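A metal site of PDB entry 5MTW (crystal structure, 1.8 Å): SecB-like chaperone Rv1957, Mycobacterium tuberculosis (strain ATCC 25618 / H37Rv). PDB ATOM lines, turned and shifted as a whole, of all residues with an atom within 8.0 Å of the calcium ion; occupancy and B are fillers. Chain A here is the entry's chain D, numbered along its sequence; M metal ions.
The side-chain carboxylate of Asp 113 lies within salt-bridge range of the guanidinium group of Arg 29, 2.5 Å away.
The calcium ion is bound by O of Tyr 114 (2.2 Å), OG of Ser 68 (2.3 Å), OD1 of Asp 113 (2.3 Å) and O of Ser 68 (2.5 Å).
The calcium ion has four donor atoms within binding distance.
Within 4 Å of the calcium ion: Ser 68, Asp 113 and Tyr 114.
The nearest printed residue that does not touch the calcium ion is His 115 (4.5 Å).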
ATOM      1  N   ARG A  25      13.666  27.677  -9.938  1.00  0.00           N
ATOM      2  CA  ARG A  25      14.417  27.978  -8.687  1.00  0.00           C
ATOM      3  C   ARG A  25      15.854  27.416  -8.593  1.00  0.00           C
ATOM      4  O   ARG A  25      16.514  27.616  -7.555  1.00  0.00           O
ATOM      5  CB  ARG A  25      13.634  27.478  -7.479  1.00  0.00           C
ATOM      6  CG  ARG A  25      12.559  28.431  -6.987  1.00  0.00           C
ATOM      7  CD  ARG A  25      11.506  27.681  -6.183  1.00  0.00           C
ATOM      8  NE  ARG A  25      10.200  28.362  -6.117  1.00  0.00           N
ATOM      9  CZ  ARG A  25       9.164  28.156  -6.927  1.00  0.00           C
ATOM     10  NH1 ARG A  25       9.231  27.308  -7.931  1.00  0.00           N
ATOM     11  NH2 ARG A  25       8.048  28.833  -6.729  1.00  0.00           N
ATOM     12  N   ARG A  29      25.975  25.050 -10.828  1.00  0.00           N
ATOM     13  CA  ARG A  29      27.141  25.506 -10.106  1.00  0.00           C
ATOM     14  C   ARG A  29      28.448  24.989 -10.734  1.00  0.00           C
ATOM     15  O   ARG A  29      29.421  25.676 -10.707  1.00  0.00           O
ATOM     16  CB  ARG A  29      27.082  25.017  -8.630  1.00  0.00           C
ATOM     17  CG  ARG A  29      26.102  25.791  -7.743  1.00  0.00           C
ATOM     18  CD  ARG A  29      26.480  27.275  -7.585  1.00  0.00           C
ATOM     19  NE  ARG A  29      25.297  28.140  -7.510  1.00  0.00           N
ATOM     20  CZ  ARG A  29      24.672  28.506  -6.389  1.00  0.00           C
ATOM     21  NH1 ARG A  29      25.113  28.131  -5.195  1.00  0.00           N
ATOM     22  NH2 ARG A  29      23.599  29.280  -6.452  1.00  0.00           N
ATOM     23  N   ILE A  67      19.599  18.389   2.008  1.00  0.00           N
ATOM     24  CA  ILE A  67      20.369  19.355   1.229  1.00  0.00           C
ATOM     25  C   ILE A  67      19.536  19.883   0.084  1.00  0.00           C
ATOM     26  O   ILE A  67      18.921  19.105  -0.671  1.00  0.00           O
ATOM     27  CB  ILE A  67      21.755  18.755   0.794  1.00  0.00           C
ATOM     28  CG1 ILE A  67      22.653  19.793   0.093  1.00  0.00           C
ATOM     29  CG2 ILE A  67      21.591  17.541  -0.101  1.00  0.00           C
ATOM     30  CD1 ILE A  67      23.941  19.182  -0.472  1.00  0.00           C
ATOM     31  N   SER A  68      19.527  21.198  -0.059  1.00  0.00           N
ATOM     32  CA  SER A  68      18.780  21.832  -1.127  1.00  0.00           C
ATOM     33  C   SER A  68      19.740  22.020  -2.370  1.00  0.00           C
ATOM     34  O   SER A  68      20.111  23.108  -2.806  1.00  0.00           O
ATOM     35  CB  SER A  68      18.130  23.143  -0.668  1.00  0.00           C
ATOM     36  OG  SER A  68      19.108  24.097  -0.321  1.00  0.00           O
ATOM     37  N   ALA A  69      20.133  20.890  -2.919  1.00  0.00           N
ATOM     38  CA  ALA A  69      21.025  20.831  -4.097  1.00  0.00           C
ATOM     39  C   ALA A  69      20.970  19.394  -4.563  1.00  0.00           C
ATOM     40  O   ALA A  69      20.590  18.527  -3.790  1.00  0.00           O
ATOM     41  CB  ALA A  69      22.450  21.159  -3.788  1.00  0.00           C
ATOM     42  N   PHE A  70      21.374  19.167  -5.795  1.00  0.00           N
ATOM     43  CA  PHE A  70      21.272  17.798  -6.392  1.00  0.00           C
ATOM     44  C   PHE A  70      22.292  17.716  -7.520  1.00  0.00           C
ATOM     45  O   PHE A  70      22.743  18.726  -8.006  1.00  0.00           O
ATOM     46  CB  PHE A  70      19.856  17.485  -6.923  1.00  0.00           C
ATOM     47  CG  PHE A  70      19.291  18.488  -7.933  1.00  0.00           C
ATOM     48  CD1 PHE A  70      18.569  19.610  -7.487  1.00  0.00           C
ATOM     49  CD2 PHE A  70      19.403  18.272  -9.294  1.00  0.00           C
ATOM     50  CE1 PHE A  70      18.099  20.532  -8.367  1.00  0.00           C
ATOM     51  CE2 PHE A  70      18.903  19.127 -10.201  1.00  0.00           C
ATOM     52  CZ  PHE A  70      18.252  20.293  -9.751  1.00  0.00           C
ATOM     53  N   PHE A 112      23.682  21.115  -9.241  1.00  0.00           N
ATOM     54  CA  PHE A 112      22.670  22.243  -9.194  1.00  0.00           C
ATOM     55  C   PHE A 112      22.352  22.565  -7.719  1.00  0.00           C
ATOM     56  O   PHE A 112      22.262  21.671  -6.909  1.00  0.00           O
ATOM     57  CB  PHE A 112      21.349  21.885  -9.882  1.00  0.00           C
ATOM     58  CG  PHE A 112      21.487  21.582 -11.354  1.00  0.00           C
ATOM     59  CD1 PHE A 112      21.932  20.352 -11.768  1.00  0.00           C
ATOM     60  CD2 PHE A 112      21.228  22.544 -12.303  1.00  0.00           C
ATOM     61  CE1 PHE A 112      22.098  20.069 -13.118  1.00  0.00           C
ATOM     62  CE2 PHE A 112      21.343  22.286 -13.660  1.00  0.00           C
ATOM     63  CZ  PHE A 112      21.819  21.069 -14.058  1.00  0.00           C
ATOM     64  N   ASP A 113      22.141  23.856  -7.466  1.00  0.00           N
ATOM     65  CA  ASP A 113      21.760  24.370  -6.192  1.00  0.00           C
ATOM     66  C   ASP A 113      20.391  24.981  -6.370  1.00  0.00           C
ATOM     67  O   ASP A 113      20.084  25.567  -7.405  1.00  0.00           O
ATOM     68  CB  ASP A 113      22.760  25.405  -5.786  1.00  0.00           C
ATOM     69  CG  ASP A 113      22.558  25.909  -4.373  1.00  0.00           C
ATOM     70  OD1 ASP A 113      21.792  25.326  -3.612  1.00  0.00           O
ATOM     71  OD2 ASP A 113      23.235  26.863  -4.033  1.00  0.00           O
ATOM     72  N   TYR A 114      19.538  24.779  -5.379  1.00  0.00           N
ATOM     73  CA  TYR A 114      18.248  25.430  -5.381  1.00  0.00           C
ATOM     74  C   TYR A 114      17.955  26.112  -4.035  1.00  0.00           C
ATOM     75  O   TYR A 114      18.587  25.799  -3.006  1.00  0.00           O
ATOM     76  CB  TYR A 114      17.158  24.469  -5.860  1.00  0.00           C
ATOM     77  CG  TYR A 114      16.768  23.313  -4.921  1.00  0.00           C
ATOM     78  CD1 TYR A 114      15.832  23.520  -3.902  1.00  0.00           C
ATOM     79  CD2 TYR A 114      17.313  22.049  -5.073  1.00  0.00           C
ATOM     80  CE1 TYR A 114      15.481  22.513  -3.072  1.00  0.00           C
ATOM     81  CE2 TYR A 114      16.988  21.015  -4.217  1.00  0.00           C
ATOM     82  CZ  TYR A 114      16.034  21.258  -3.217  1.00  0.00           C
ATOM     83  OH  TYR A 114      15.625  20.225  -2.397  1.00  0.00           O
ATOM     84  N   HIS A 115      17.048  27.085  -4.171  1.00  0.00           N
ATOM     85  CA  HIS A 115      16.490  27.978  -3.147  1.00  0.00           C
ATOM     86  C   HIS A 115      14.966  27.732  -3.058  1.00  0.00           C
ATOM     87  O   HIS A 115      14.256  27.818  -4.075  1.00  0.00           O
ATOM     88  CB  HIS A 115      16.701  29.420  -3.607  1.00  0.00           C
ATOM     89  CG  HIS A 115      16.577  30.445  -2.517  1.00  0.00           C
ATOM     90  ND1 HIS A 115      15.556  30.442  -1.581  1.00  0.00           N
ATOM     91  CD2 HIS A 115      17.336  31.539  -2.246  1.00  0.00           C
ATOM     92  CE1 HIS A 115      15.709  31.467  -0.771  1.00  0.00           C
ATOM     93  NE2 HIS A 115      16.786  32.142  -1.146  1.00  0.00           N
ATOM     94  N   LEU A 116      14.499  27.466  -1.854  1.00  0.00           N
ATOM     95  CA  LEU A 116      13.045  27.341  -1.520  1.00  0.00           C
ATOM     96  C   LEU A 116      12.569  28.457  -0.550  1.00  0.00           C
ATOM     97  O   LEU A 116      13.238  28.705   0.463  1.00  0.00           O
ATOM     98  CB  LEU A 116      12.788  25.975  -0.871  1.00  0.00           C
ATOM     99  CG  LEU A 116      12.010  24.906  -1.674  1.00  0.00           C
ATOM    100  CD1 LEU A 116      12.238  24.972  -3.183  1.00  0.00           C
ATOM    101  CD2 LEU A 116      12.258  23.519  -1.102  1.00  0.00           C
HETATM  102 CA    CA M   1      20.386  25.339  -1.759  1.00  0.00          CA
